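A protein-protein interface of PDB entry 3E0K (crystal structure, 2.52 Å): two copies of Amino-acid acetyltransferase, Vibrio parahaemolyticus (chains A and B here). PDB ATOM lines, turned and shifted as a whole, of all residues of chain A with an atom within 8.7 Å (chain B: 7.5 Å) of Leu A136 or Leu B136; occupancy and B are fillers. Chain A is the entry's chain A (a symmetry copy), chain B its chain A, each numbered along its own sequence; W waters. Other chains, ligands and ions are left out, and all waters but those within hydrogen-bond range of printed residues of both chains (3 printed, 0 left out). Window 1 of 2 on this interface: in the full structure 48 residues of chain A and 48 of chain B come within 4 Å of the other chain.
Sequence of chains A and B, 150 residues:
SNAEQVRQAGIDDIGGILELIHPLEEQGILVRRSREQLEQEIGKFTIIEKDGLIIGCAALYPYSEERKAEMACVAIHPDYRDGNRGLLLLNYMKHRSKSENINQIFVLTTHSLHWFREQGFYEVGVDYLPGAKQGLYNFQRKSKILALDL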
ATOM      1  N   ILE A  29     -31.477   7.052 -21.993  1.00  0.00           N
ATOM      2  CA  ILE A  29     -30.924   6.338 -20.841  1.00  0.00           C
ATOM      3  C   ILE A  29     -29.980   5.168 -21.218  1.00  0.00           C
ATOM      4  O   ILE A  29     -28.869   5.089 -20.695  1.00  0.00           O
ATOM      5  CB  ILE A  29     -32.059   5.866 -19.866  1.00  0.00           C
ATOM      6  CG1 ILE A  29     -32.936   7.056 -19.445  1.00  0.00           C
ATOM      7  CG2 ILE A  29     -31.475   5.150 -18.636  1.00  0.00           C
ATOM      8  CD1 ILE A  29     -34.142   6.678 -18.598  1.00  0.00           C
ATOM      9  N   LEU A  30     -30.418   4.278 -22.111  1.00  0.00           N
ATOM     10  CA  LEU A  30     -29.668   3.066 -22.464  1.00  0.00           C
ATOM     11  C   LEU A  30     -29.020   3.150 -23.845  1.00  0.00           C
ATOM     12  O   LEU A  30     -28.171   2.322 -24.209  1.00  0.00           O
ATOM     13  CB  LEU A  30     -30.579   1.838 -22.385  1.00  0.00           C
ATOM     14  CG  LEU A  30     -30.523   0.908 -21.164  1.00  0.00           C
ATOM     15  CD1 LEU A  30     -30.167   1.607 -19.861  1.00  0.00           C
ATOM     16  CD2 LEU A  30     -31.840   0.195 -21.025  1.00  0.00           C
ATOM     17  N   ARG A  33     -30.203  -1.771 -27.173  1.00  0.00           N
ATOM     18  CA  ARG A  33     -30.136  -3.233 -27.393  1.00  0.00           C
ATOM     19  C   ARG A  33     -31.037  -3.730 -28.531  1.00  0.00           C
ATOM     20  O   ARG A  33     -32.274  -3.690 -28.416  1.00  0.00           O
ATOM     21  CB  ARG A  33     -30.440  -4.007 -26.085  1.00  0.00           C
ATOM     22  CG  ARG A  33     -29.207  -4.169 -25.191  1.00  0.00           C
ATOM     23  CD  ARG A  33     -29.520  -4.639 -23.800  1.00  0.00           C
ATOM     24  NE  ARG A  33     -28.337  -4.717 -22.944  1.00  0.00           N
ATOM     25  CZ  ARG A  33     -27.808  -3.673 -22.306  1.00  0.00           C
ATOM     26  NH1 ARG A  33     -28.338  -2.474 -22.460  1.00  0.00           N
ATOM     27  NH2 ARG A  33     -26.741  -3.817 -21.523  1.00  0.00           N
ATOM     28  N   TYR A  61     -23.421  -8.359 -15.120  1.00  0.00           N
ATOM     29  CA  TYR A  61     -22.209  -8.647 -15.884  1.00  0.00           C
ATOM     30  C   TYR A  61     -21.055  -8.953 -14.954  1.00  0.00           C
ATOM     31  O   TYR A  61     -20.472  -8.038 -14.364  1.00  0.00           O
ATOM     32  CB  TYR A  61     -21.837  -7.482 -16.782  1.00  0.00           C
ATOM     33  CG  TYR A  61     -22.883  -7.202 -17.805  1.00  0.00           C
ATOM     34  CD1 TYR A  61     -23.027  -8.016 -18.931  1.00  0.00           C
ATOM     35  CD2 TYR A  61     -23.734  -6.126 -17.661  1.00  0.00           C
ATOM     36  CE1 TYR A  61     -24.002  -7.749 -19.895  1.00  0.00           C
ATOM     37  CE2 TYR A  61     -24.694  -5.846 -18.614  1.00  0.00           C
ATOM     38  CZ  TYR A  61     -24.829  -6.664 -19.725  1.00  0.00           C
ATOM     39  OH  TYR A  61     -25.792  -6.359 -20.663  1.00  0.00           O
ATOM     40  N   TYR A  63     -17.486  -9.841 -13.343  1.00  0.00           N
ATOM     41  CA  TYR A  63     -16.053  -9.729 -13.552  1.00  0.00           C
ATOM     42  C   TYR A  63     -15.412 -10.677 -12.573  1.00  0.00           C
ATOM     43  O   TYR A  63     -15.124 -10.326 -11.420  1.00  0.00           O
ATOM     44  CB  TYR A  63     -15.580  -8.293 -13.361  1.00  0.00           C
ATOM     45  CG  TYR A  63     -16.098  -7.433 -14.470  1.00  0.00           C
ATOM     46  CD1 TYR A  63     -15.339  -7.243 -15.631  1.00  0.00           C
ATOM     47  CD2 TYR A  63     -17.380  -6.862 -14.403  1.00  0.00           C
ATOM     48  CE1 TYR A  63     -15.823  -6.481 -16.682  1.00  0.00           C
ATOM     49  CE2 TYR A  63     -17.887  -6.104 -15.468  1.00  0.00           C
ATOM     50  CZ  TYR A  63     -17.094  -5.920 -16.593  1.00  0.00           C
ATOM     51  OH  TYR A  63     -17.539  -5.169 -17.638  1.00  0.00           O
ATOM     52  N   GLU A  70     -21.316  -5.860 -12.568  1.00  0.00           N
ATOM     53  CA  GLU A  70     -22.121  -4.691 -12.825  1.00  0.00           C
ATOM     54  C   GLU A  70     -23.562  -5.086 -13.023  1.00  0.00           C
ATOM     55  O   GLU A  70     -23.869  -5.968 -13.826  1.00  0.00           O
ATOM     56  CB  GLU A  70     -21.653  -3.972 -14.079  1.00  0.00           C
ATOM     57  CG  GLU A  70     -22.497  -2.742 -14.376  1.00  0.00           C
ATOM     58  CD  GLU A  70     -22.042  -1.990 -15.617  1.00  0.00           C
ATOM     59  OE1 GLU A  70     -21.023  -2.446 -16.215  1.00  0.00           O
ATOM     60  OE2 GLU A  70     -22.700  -0.958 -15.976  1.00  0.00           O
ATOM     61  N   ALA A  72     -26.736  -3.745 -14.629  1.00  0.00           N
ATOM     62  CA  ALA A  72     -27.112  -2.752 -15.616  1.00  0.00           C
ATOM     63  C   ALA A  72     -28.503  -3.037 -16.153  1.00  0.00           C
ATOM     64  O   ALA A  72     -29.092  -4.082 -15.860  1.00  0.00           O
ATOM     65  CB  ALA A  72     -26.117  -2.754 -16.759  1.00  0.00           C
ATOM     66  N   PHE A 106     -21.595  -3.162  -8.724  1.00  0.00           N
ATOM     67  CA  PHE A 106     -21.499  -1.754  -9.029  1.00  0.00           C
ATOM     68  C   PHE A 106     -22.452  -1.372 -10.114  1.00  0.00           C
ATOM     69  O   PHE A 106     -22.843  -2.198 -10.926  1.00  0.00           O
ATOM     70  CB  PHE A 106     -20.072  -1.350  -9.401  1.00  0.00           C
ATOM     71  CG  PHE A 106     -19.550  -1.967 -10.686  1.00  0.00           C
ATOM     72  CD1 PHE A 106     -19.658  -1.289 -11.893  1.00  0.00           C
ATOM     73  CD2 PHE A 106     -18.881  -3.204 -10.670  1.00  0.00           C
ATOM     74  CE1 PHE A 106     -19.133  -1.848 -13.083  1.00  0.00           C
ATOM     75  CE2 PHE A 106     -18.352  -3.768 -11.836  1.00  0.00           C
ATOM     76  CZ  PHE A 106     -18.476  -3.088 -13.046  1.00  0.00           C
ATOM     77  N   LEU A 108     -23.460   2.105 -12.858  1.00  0.00           N
ATOM     78  CA  LEU A 108     -23.095   3.404 -13.442  1.00  0.00           C
ATOM     79  C   LEU A 108     -24.390   4.131 -13.617  1.00  0.00           C
ATOM     80  O   LEU A 108     -25.250   3.684 -14.367  1.00  0.00           O
ATOM     81  CB  LEU A 108     -22.434   3.212 -14.799  1.00  0.00           C
ATOM     82  CG  LEU A 108     -20.958   2.795 -14.785  1.00  0.00           C
ATOM     83  CD1 LEU A 108     -20.618   1.652 -13.821  1.00  0.00           C
ATOM     84  CD2 LEU A 108     -20.539   2.422 -16.198  1.00  0.00           C
ATOM     85  N   VAL A 126     -13.069   6.101 -11.142  1.00  0.00           N
ATOM     86  CA  VAL A 126     -12.958   5.258 -12.350  1.00  0.00           C
ATOM     87  C   VAL A 126     -11.927   4.169 -12.224  1.00  0.00           C
ATOM     88  O   VAL A 126     -12.063   3.131 -12.854  1.00  0.00           O
ATOM     89  CB  VAL A 126     -12.642   6.038 -13.640  1.00  0.00           C
ATOM     90  CG1 VAL A 126     -13.920   6.670 -14.234  1.00  0.00           C
ATOM     91  CG2 VAL A 126     -11.534   7.062 -13.397  1.00  0.00           C
ATOM     92  N   LEU A 129     -13.101   0.546 -11.514  1.00  0.00           N
ATOM     93  CA  LEU A 129     -13.641  -0.308 -12.583  1.00  0.00           C
ATOM     94  C   LEU A 129     -12.701  -1.436 -13.019  1.00  0.00           C
ATOM     95  O   LEU A 129     -11.482  -1.235 -13.172  1.00  0.00           O
ATOM     96  CB  LEU A 129     -14.073   0.524 -13.795  1.00  0.00           C
ATOM     97  CG  LEU A 129     -15.190   1.551 -13.523  1.00  0.00           C
ATOM     98  CD1 LEU A 129     -15.458   2.446 -14.724  1.00  0.00           C
ATOM     99  CD2 LEU A 129     -16.484   0.893 -13.063  1.00  0.00           C
ATOM    100  N   PRO A 130     -13.264  -2.636 -13.230  1.00  0.00           N
ATOM    101  CA  PRO A 130     -12.451  -3.748 -13.723  1.00  0.00           C
ATOM    102  C   PRO A 130     -11.868  -3.366 -15.076  1.00  0.00           C
ATOM    103  O   PRO A 130     -12.618  -2.850 -15.917  1.00  0.00           O
ATOM    104  CB  PRO A 130     -13.462  -4.874 -13.905  1.00  0.00           C
ATOM    105  CG  PRO A 130     -14.584  -4.520 -13.060  1.00  0.00           C
ATOM    106  CD  PRO A 130     -14.665  -3.025 -13.046  1.00  0.00           C
ATOM    107  N   GLY A 131     -10.562  -3.615 -15.275  1.00  0.00           N
ATOM    108  CA  GLY A 131      -9.820  -3.203 -16.483  1.00  0.00           C
ATOM    109  C   GLY A 131     -10.556  -3.269 -17.814  1.00  0.00           C
ATOM    110  O   GLY A 131     -10.363  -2.417 -18.684  1.00  0.00           O
ATOM    111  N   ALA A 132     -11.402  -4.275 -17.987  1.00  0.00           N
ATOM    112  CA  ALA A 132     -12.116  -4.413 -19.251  1.00  0.00           C
ATOM    113  C   ALA A 132     -13.003  -3.202 -19.467  1.00  0.00           C
ATOM    114  O   ALA A 132     -13.091  -2.671 -20.576  1.00  0.00           O
ATOM    115  CB  ALA A 132     -12.948  -5.678 -19.268  1.00  0.00           C
ATOM    116  N   LYS A 133     -13.622  -2.762 -18.372  1.00  0.00           N
ATOM    117  CA  LYS A 133     -14.615  -1.703 -18.363  1.00  0.00           C
ATOM    118  C   LYS A 133     -13.952  -0.310 -18.273  1.00  0.00           C
ATOM    119  O   LYS A 133     -14.652   0.718 -18.282  1.00  0.00           O
ATOM    120  CB  LYS A 133     -15.590  -1.927 -17.190  1.00  0.00           C
ATOM    121  CG  LYS A 133     -17.083  -1.982 -17.576  1.00  0.00           C
ATOM    122  CD  LYS A 133     -17.737  -0.606 -17.645  1.00  0.00           C
ATOM    123  CE  LYS A 133     -19.257  -0.671 -17.502  1.00  0.00           C
ATOM    124  NZ  LYS A 133     -20.052  -0.829 -18.781  1.00  0.00           N
ATOM    125  N   GLN A 134     -12.614  -0.278 -18.206  1.00  0.00           N
ATOM    126  CA  GLN A 134     -11.863   0.985 -18.143  1.00  0.00           C
ATOM    127  C   GLN A 134     -11.735   1.721 -19.484  1.00  0.00           C
ATOM    128  O   GLN A 134     -11.960   2.933 -19.542  1.00  0.00           O
ATOM    129  CB  GLN A 134     -10.486   0.799 -17.491  1.00  0.00           C
ATOM    130  CG  GLN A 134     -10.433   1.264 -16.021  1.00  0.00           C
ATOM    131  CD  GLN A 134      -9.224   0.710 -15.268  1.00  0.00           C
ATOM    132  OE1 GLN A 134      -8.225   0.308 -15.883  1.00  0.00           O
ATOM    133  NE2 GLN A 134      -9.313   0.679 -13.939  1.00  0.00           N
ATOM    134  N   GLY A 135     -11.380   1.000 -20.547  1.00  0.00           N
ATOM    135  CA  GLY A 135     -11.307   1.595 -21.894  1.00  0.00           C
ATOM    136  C   GLY A 135     -12.504   2.467 -22.285  1.00  0.00           C
ATOM    137  O   GLY A 135     -12.362   3.399 -23.090  1.00  0.00           O
ATOM    138  N   LEU A 136     -13.668   2.178 -21.689  1.00  0.00           N
ATOM    139  CA  LEU A 136     -14.947   2.816 -22.033  1.00  0.00           C
ATOM    140  C   LEU A 136     -15.355   4.022 -21.172  1.00  0.00           C
ATOM    141  O   LEU A 136     -15.920   4.996 -21.710  1.00  0.00           O
ATOM    142  CB  LEU A 136     -16.058   1.789 -22.027  1.00  0.00           C
ATOM    143  N   TYR A 137     -15.103   3.952 -19.855  1.00  0.00           N
ATOM    144  CA  TYR A 137     -15.402   5.062 -18.929  1.00  0.00           C
ATOM    145  C   TYR A 137     -14.651   6.320 -19.352  1.00  0.00           C
ATOM    146  O   TYR A 137     -15.191   7.421 -19.296  1.00  0.00           O
ATOM    147  CB  TYR A 137     -15.064   4.684 -17.488  1.00  0.00           C
ATOM    148  N   ASN A 138     -13.415   6.132 -19.809  1.00  0.00           N
ATOM    149  CA  ASN A 138     -12.579   7.222 -20.278  1.00  0.00           C
ATOM    150  C   ASN A 138     -12.751   7.462 -21.783  1.00  0.00           C
ATOM    151  O   ASN A 138     -11.795   7.848 -22.459  1.00  0.00           O
ATOM    152  CB  ASN A 138     -11.107   6.957 -19.914  1.00  0.00           C
ATOM    153  N   PHE A 139     -13.973   7.247 -22.283  1.00  0.00           N
ATOM    154  CA  PHE A 139     -14.347   7.463 -23.703  1.00  0.00           C
ATOM    155  C   PHE A 139     -13.638   8.662 -24.364  1.00  0.00           C
ATOM    156  O   PHE A 139     -14.243   9.688 -24.686  1.00  0.00           O
ATOM    157  CB  PHE A 139     -15.881   7.577 -23.846  1.00  0.00           C
ATOM    158  CG  PHE A 139     -16.398   7.344 -25.252  1.00  0.00           C
ATOM    159  CD1 PHE A 139     -16.807   8.422 -26.051  1.00  0.00           C
ATOM    160  CD2 PHE A 139     -16.501   6.050 -25.774  1.00  0.00           C
ATOM    161  CE1 PHE A 139     -17.295   8.213 -27.356  1.00  0.00           C
ATOM    162  CE2 PHE A 139     -16.987   5.830 -27.075  1.00  0.00           C
ATOM    163  CZ  PHE A 139     -17.386   6.910 -27.865  1.00  0.00           C
ATOM    164  N   ARG A 141     -15.333  11.775 -26.352  1.00  0.00           N
ATOM    165  CA  ARG A 141     -15.790  12.831 -27.296  1.00  0.00           C
ATOM    166  C   ARG A 141     -15.331  12.575 -28.748  1.00  0.00           C
ATOM    167  O   ARG A 141     -16.074  11.968 -29.528  1.00  0.00           O
ATOM    168  CB  ARG A 141     -15.420  14.253 -26.820  1.00  0.00           C
ATOM    169  CG  ARG A 141     -13.981  14.423 -26.312  1.00  0.00           C
ATOM    170  CD  ARG A 141     -13.775  15.807 -25.716  1.00  0.00           C
ATOM    171  NE  ARG A 141     -13.330  16.760 -26.730  1.00  0.00           N
ATOM    172  CZ  ARG A 141     -13.571  18.072 -26.708  1.00  0.00           C
ATOM    173  NH1 ARG A 141     -14.278  18.616 -25.720  1.00  0.00           N
ATOM    174  NH2 ARG A 141     -13.111  18.845 -27.685  1.00  0.00           N
ATOM    175  N   SER A 143     -13.790  10.280 -29.760  1.00  0.00           N
ATOM    176  CA  SER A 143     -13.376   8.902 -29.434  1.00  0.00           C
ATOM    177  C   SER A 143     -14.075   7.818 -30.298  1.00  0.00           C
ATOM    178  O   SER A 143     -15.284   7.592 -30.193  1.00  0.00           O
ATOM    179  CB  SER A 143     -13.602   8.657 -27.932  1.00  0.00           C
ATOM    180  OG  SER A 143     -13.129   7.390 -27.523  1.00  0.00           O
ATOM    181  N   ILE A 145     -14.899   4.055 -32.140  1.00  0.00           N
ATOM    182  CA  ILE A 145     -14.932   2.617 -32.003  1.00  0.00           C
ATOM    183  C   ILE A 145     -14.601   2.004 -33.365  1.00  0.00           C
ATOM    184  O   ILE A 145     -15.310   2.236 -34.343  1.00  0.00           O
ATOM    185  CB  ILE A 145     -16.334   2.106 -31.574  1.00  0.00           C
ATOM    186  CG1 ILE A 145     -16.855   2.874 -30.357  1.00  0.00           C
ATOM    187  CG2 ILE A 145     -16.312   0.578 -31.303  1.00  0.00           C
ATOM    188  CD1 ILE A 145     -18.383   2.783 -30.179  1.00  0.00           C
ATOM    189  N   TYR B  63     -15.561 -11.137 -25.628  1.00  0.00           N
ATOM    190  CA  TYR B  63     -16.998 -11.170 -25.429  1.00  0.00           C
ATOM    191  C   TYR B  63     -17.495 -12.392 -26.156  1.00  0.00           C
ATOM    192  O   TYR B  63     -17.809 -12.354 -27.354  1.00  0.00           O
ATOM    193  CB  TYR B  63     -17.653  -9.890 -25.935  1.00  0.00           C
ATOM    194  CG  TYR B  63     -17.269  -8.740 -25.059  1.00  0.00           C
ATOM    195  CD1 TYR B  63     -18.065  -8.391 -23.960  1.00  0.00           C
ATOM    196  CD2 TYR B  63     -16.072  -8.036 -25.274  1.00  0.00           C
ATOM    197  CE1 TYR B  63     -17.700  -7.353 -23.119  1.00  0.00           C
ATOM    198  CE2 TYR B  63     -15.685  -6.995 -24.417  1.00  0.00           C
ATOM    199  CZ  TYR B  63     -16.513  -6.665 -23.352  1.00  0.00           C
ATOM    200  OH  TYR B  63     -16.187  -5.644 -22.513  1.00  0.00           O
ATOM    201  N   GLU B  70     -12.274  -6.971 -27.348  1.00  0.00           N
ATOM    202  CA  GLU B  70     -11.634  -5.679 -27.377  1.00  0.00           C
ATOM    203  C   GLU B  70     -10.157  -5.825 -27.117  1.00  0.00           C
ATOM    204  O   GLU B  70      -9.748  -6.453 -26.138  1.00  0.00           O
ATOM    205  CB  GLU B  70     -12.211  -4.761 -26.313  1.00  0.00           C
ATOM    206  CG  GLU B  70     -11.541  -3.395 -26.317  1.00  0.00           C
ATOM    207  CD  GLU B  70     -12.109  -2.447 -25.274  1.00  0.00           C
ATOM    208  OE1 GLU B  70     -13.068  -2.884 -24.572  1.00  0.00           O
ATOM    209  OE2 GLU B  70     -11.598  -1.283 -25.169  1.00  0.00           O
ATOM    210  N   LEU B 108     -11.199   1.061 -28.914  1.00  0.00           N
ATOM    211  CA  LEU B 108     -11.740   2.400 -28.636  1.00  0.00           C
ATOM    212  C   LEU B 108     -10.555   3.311 -28.652  1.00  0.00           C
ATOM    213  O   LEU B 108      -9.655   3.164 -27.833  1.00  0.00           O
ATOM    214  CB  LEU B 108     -12.391   2.438 -27.262  1.00  0.00           C
ATOM    215  CG  LEU B 108     -13.799   1.838 -27.158  1.00  0.00           C
ATOM    216  CD1 LEU B 108     -13.971   0.471 -27.830  1.00  0.00           C
ATOM    217  CD2 LEU B 108     -14.187   1.745 -25.691  1.00  0.00           C
ATOM    218  N   LEU B 129     -21.243  -2.108 -29.710  1.00  0.00           N
ATOM    219  CA  LEU B 129     -20.611  -2.618 -28.483  1.00  0.00           C
ATOM    220  C   LEU B 129     -21.401  -3.730 -27.786  1.00  0.00           C
ATOM    221  O   LEU B 129     -22.638  -3.662 -27.666  1.00  0.00           O
ATOM    222  CB  LEU B 129     -20.311  -1.482 -27.499  1.00  0.00           C
ATOM    223  CG  LEU B 129     -19.334  -0.407 -28.015  1.00  0.00           C
ATOM    224  CD1 LEU B 129     -19.204   0.765 -27.054  1.00  0.00           C
ATOM    225  CD2 LEU B 129     -17.957  -0.977 -28.333  1.00  0.00           C
ATOM    226  N   GLY B 131     -23.269  -5.600 -25.061  1.00  0.00           N
ATOM    227  CA  GLY B 131     -24.078  -5.024 -23.968  1.00  0.00           C
ATOM    228  C   GLY B 131     -23.360  -4.687 -22.668  1.00  0.00           C
ATOM    229  O   GLY B 131     -23.676  -3.693 -22.012  1.00  0.00           O
ATOM    230  N   ALA B 132     -22.392  -5.508 -22.283  1.00  0.00           N
ATOM    231  CA  ALA B 132     -21.685  -5.259 -21.032  1.00  0.00           C
ATOM    232  C   ALA B 132     -20.969  -3.925 -21.111  1.00  0.00           C
ATOM    233  O   ALA B 132     -20.967  -3.149 -20.154  1.00  0.00           O
ATOM    234  CB  ALA B 132     -20.695  -6.367 -20.740  1.00  0.00           C
ATOM    235  N   LYS B 133     -20.396  -3.669 -22.287  1.00  0.00           N
ATOM    236  CA  LYS B 133     -19.551  -2.518 -22.553  1.00  0.00           C
ATOM    237  C   LYS B 133     -20.390  -1.282 -22.947  1.00  0.00           C
ATOM    238  O   LYS B 133     -19.830  -0.197 -23.183  1.00  0.00           O
ATOM    239  CB  LYS B 133     -18.537  -2.874 -23.658  1.00  0.00           C
ATOM    240  CG  LYS B 133     -17.056  -2.644 -23.293  1.00  0.00           C
ATOM    241  CD  LYS B 133     -16.589  -1.214 -23.549  1.00  0.00           C
ATOM    242  CE  LYS B 133     -15.071  -1.110 -23.696  1.00  0.00           C
ATOM    243  NZ  LYS B 133     -14.282  -0.867 -22.427  1.00  0.00           N
ATOM    244  N   GLN B 134     -21.718  -1.442 -22.999  1.00  0.00           N
ATOM    245  CA  GLN B 134     -22.628  -0.337 -23.338  1.00  0.00           C
ATOM    246  C   GLN B 134     -22.871   0.662 -22.197  1.00  0.00           C
ATOM    247  O   GLN B 134     -22.809   1.874 -22.421  1.00  0.00           O
ATOM    248  CB  GLN B 134     -23.959  -0.846 -23.909  1.00  0.00           C
ATOM    249  CG  GLN B 134     -24.050  -0.739 -25.445  1.00  0.00           C
ATOM    250  CD  GLN B 134     -25.164  -1.604 -26.033  1.00  0.00           C
ATOM    251  OE1 GLN B 134     -26.110  -1.982 -25.328  1.00  0.00           O
ATOM    252  NE2 GLN B 134     -25.052  -1.925 -27.322  1.00  0.00           N
ATOM    253  N   GLY B 135     -23.145   0.163 -20.993  1.00  0.00           N
ATOM    254  CA  GLY B 135     -23.316   1.034 -19.816  1.00  0.00           C
ATOM    255  C   GLY B 135     -22.250   2.122 -19.652  1.00  0.00           C
ATOM    256  O   GLY B 135     -22.525   3.186 -19.079  1.00  0.00           O
ATOM    257  N   LEU B 136     -21.050   1.860 -20.185  1.00  0.00           N
ATOM    258  CA  LEU B 136     -19.871   2.722 -20.015  1.00  0.00           C
ATOM    259  C   LEU B 136     -19.611   3.742 -21.133  1.00  0.00           C
ATOM    260  O   LEU B 136     -19.187   4.879 -20.841  1.00  0.00           O
ATOM    261  CB  LEU B 136     -18.634   1.875 -19.803  1.00  0.00           C
ATOM    262  N   TYR B 137     -19.832   3.341 -22.396  1.00  0.00           N
ATOM    263  CA  TYR B 137     -19.667   4.240 -23.555  1.00  0.00           C
ATOM    264  C   TYR B 137     -20.583   5.452 -23.419  1.00  0.00           C
ATOM    265  O   TYR B 137     -20.191   6.572 -23.732  1.00  0.00           O
ATOM    266  CB  TYR B 137     -19.931   3.503 -24.867  1.00  0.00           C
ATOM    267  N   ASN B 138     -21.790   5.212 -22.912  1.00  0.00           N
ATOM    268  CA  ASN B 138     -22.769   6.261 -22.691  1.00  0.00           C
ATOM    269  C   ASN B 138     -22.653   6.859 -21.283  1.00  0.00           C
ATOM    270  O   ASN B 138     -23.662   7.259 -20.698  1.00  0.00           O
ATOM    271  CB  ASN B 138     -24.188   5.730 -22.963  1.00  0.00           C
ATOM    272  N   PHE B 139     -21.421   6.925 -20.766  1.00  0.00           N
ATOM    273  CA  PHE B 139     -21.101   7.507 -19.438  1.00  0.00           C
ATOM    274  C   PHE B 139     -21.971   8.721 -19.058  1.00  0.00           C
ATOM    275  O   PHE B 139     -21.510   9.863 -18.987  1.00  0.00           O
ATOM    276  CB  PHE B 139     -19.598   7.851 -19.349  1.00  0.00           C
ATOM    277  CG  PHE B 139     -19.076   8.014 -17.934  1.00  0.00           C
ATOM    278  CD1 PHE B 139     -18.824   9.290 -17.409  1.00  0.00           C
ATOM    279  CD2 PHE B 139     -18.811   6.898 -17.134  1.00  0.00           C
ATOM    280  CE1 PHE B 139     -18.333   9.450 -16.098  1.00  0.00           C
ATOM    281  CE2 PHE B 139     -18.321   7.046 -15.824  1.00  0.00           C
ATOM    282  CZ  PHE B 139     -18.079   8.321 -15.307  1.00  0.00           C
ATOM    283  N   SER B 143     -22.114  11.532 -14.175  1.00  0.00           N
ATOM    284  CA  SER B 143     -22.339  10.074 -14.173  1.00  0.00           C
ATOM    285  C   SER B 143     -21.518   9.316 -13.095  1.00  0.00           C
ATOM    286  O   SER B 143     -20.287   9.233 -13.164  1.00  0.00           O
ATOM    287  CB  SER B 143     -22.060   9.525 -15.582  1.00  0.00           C
ATOM    288  OG  SER B 143     -22.357   8.147 -15.685  1.00  0.00           O
HETATM  289  O   HOH W   1     -20.099  -4.730 -17.294  1.00  0.00           O
HETATM  290  O   HOH W   2     -13.701  -4.963 -22.986  1.00  0.00           O
HETATM  291  O   HOH W   3     -25.953  -1.348 -20.282  1.00  0.00           O
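The side-chain amino group (NZ) of Lys B133 is in salt-bridge range of the side-chain carboxylate (OE1) of Glu B70.
The backbone carbonyl oxygen (O) of Leu B129 lies within hydrogen-bond range of the side-chain amide nitrogen (NE2) of Gln B134 (3.0 Å).
NH2 of Arg A33 lies within hydrogen-bond range of OH of Tyr A61 (2.8 Å).
The backbone carbonyl oxygen (O) of Glu A70 is in hydrogen-bond range of the backbone NH (N) of Tyr A61 (2.8 Å).
NZ of Lys A133 is in salt-bridge range of OE1 of Glu A70.
Water W2 lies within hydrogen-bond range of OH of Tyr B63, OE1 of Glu B70 and O of Ala A132.
Water W1 lies within hydrogen-bond range of the side-chain hydroxyl (OH) of Tyr A63 (2.6 Å), the side-chain carboxylate (OE1) of Glu A70 (2.7 Å) and the backbone carbonyl oxygen (O) of Ala B132 (3.4 Å).
Water W3 lies within hydrogen-bond range of NH2 of Arg A33 (2.9 Å) and N of Gly B135 (3.3 Å).
Of chain B, only Leu B108, Lys B133 and Leu B136 come within 4 Å of Leu A136.
Gly A135 touches just these residues of chain B: Leu B108 and Lys B133.
Tyr B137 touches none of the printed residues of chain A.
Of the printed residues of chain B, Ala A132 touches Lys B133.
Printed residues of chain A within 4 Å of Gly B131: Arg A33 (3.1 Å) and Tyr A61 (3.6 Å).
The nearest residue of chain A that does not touch Leu B136 is Tyr A137 (4.1 Å).
Of the 24 printed residues of chain A, 8 touch a printed residue of chain B.
Along chain A the printed residues that touch a printed residue of chain B span positions 33 to 145.
Of the 14 printed residues of chain B, 8 touch a printed residue of chain A.
Hydrophobic or aromatic side chains of chain B within 4 Å of the printed part of chain A: Leu B108, Leu B129, Ala B132 and Leu B136.
Along chain B the printed residues that touch a printed residue of chain A span positions 108 to 136.
Among the printed residues, 16 pairs touch across the chains.
Among the printed residues, no Asp or Glu carboxylate lies within 4 Å of a Lys or Arg side-chain nitrogen of the other chain.
The backbone carbonyl oxygen (O) of Gly B131 lies within hydrogen-bond range of the guanidinium group (NH2) of Arg A33 (3.1 Å).
NZ of Lys A133 is in hydrogen-bond range of O of Ala B132 (2.8 Å).
The side-chain amino group (NZ) of Lys B133 lies within hydrogen-bond range of the backbone carbonyl oxygen (O) of Ala A132, 2.8 Å away.
The side-chain amino group of Lys A133 sits close to the backbone NH of Leu B136 (3.2 Å).
The backbone NH (N) of Leu A136 sits close to the side-chain amino group (NZ) of Lys B133 (3.2 Å).
The backbone carbonyl oxygen of Leu A136 sits close to the backbone carbonyl oxygen of Leu B136 (3.4 Å).
Among the printed residues, merely in contact across the chains: Tyr A61 with Ala B132 (3.4 Å), Tyr A61 with Gly B131 (3.6 Å), Leu A108 with Gly B135 (3.6 Å), Gly A135 with Leu B108 (3.6 Å), Arg A33 with Gln B134 (3.7 Å), Ile A145 with Leu B129 (3.7 Å), Gly A135 with Lys B133 (3.8 Å), Lys A133 with Gly B135 (3.8 Å), Leu A136 with Leu B108 (3.9 Å) and Leu A108 with Leu B136 (3.9 Å).
Leu A108 touches Gly B135, and with the chains exchanged Gly A135 touches Leu B108.
Ala A132 touches Lys B133, and with the chains exchanged Lys A133 touches Ala B132.
Lys A133 touches Gly B135, and with the chains exchanged Gly A135 touches Lys B133.
Leu A136 touches its own counterpart, Leu B136.
Of the 16 pairs that touch across the chains among the printed residues, 11 have their exchanged pair printed and touching as well.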
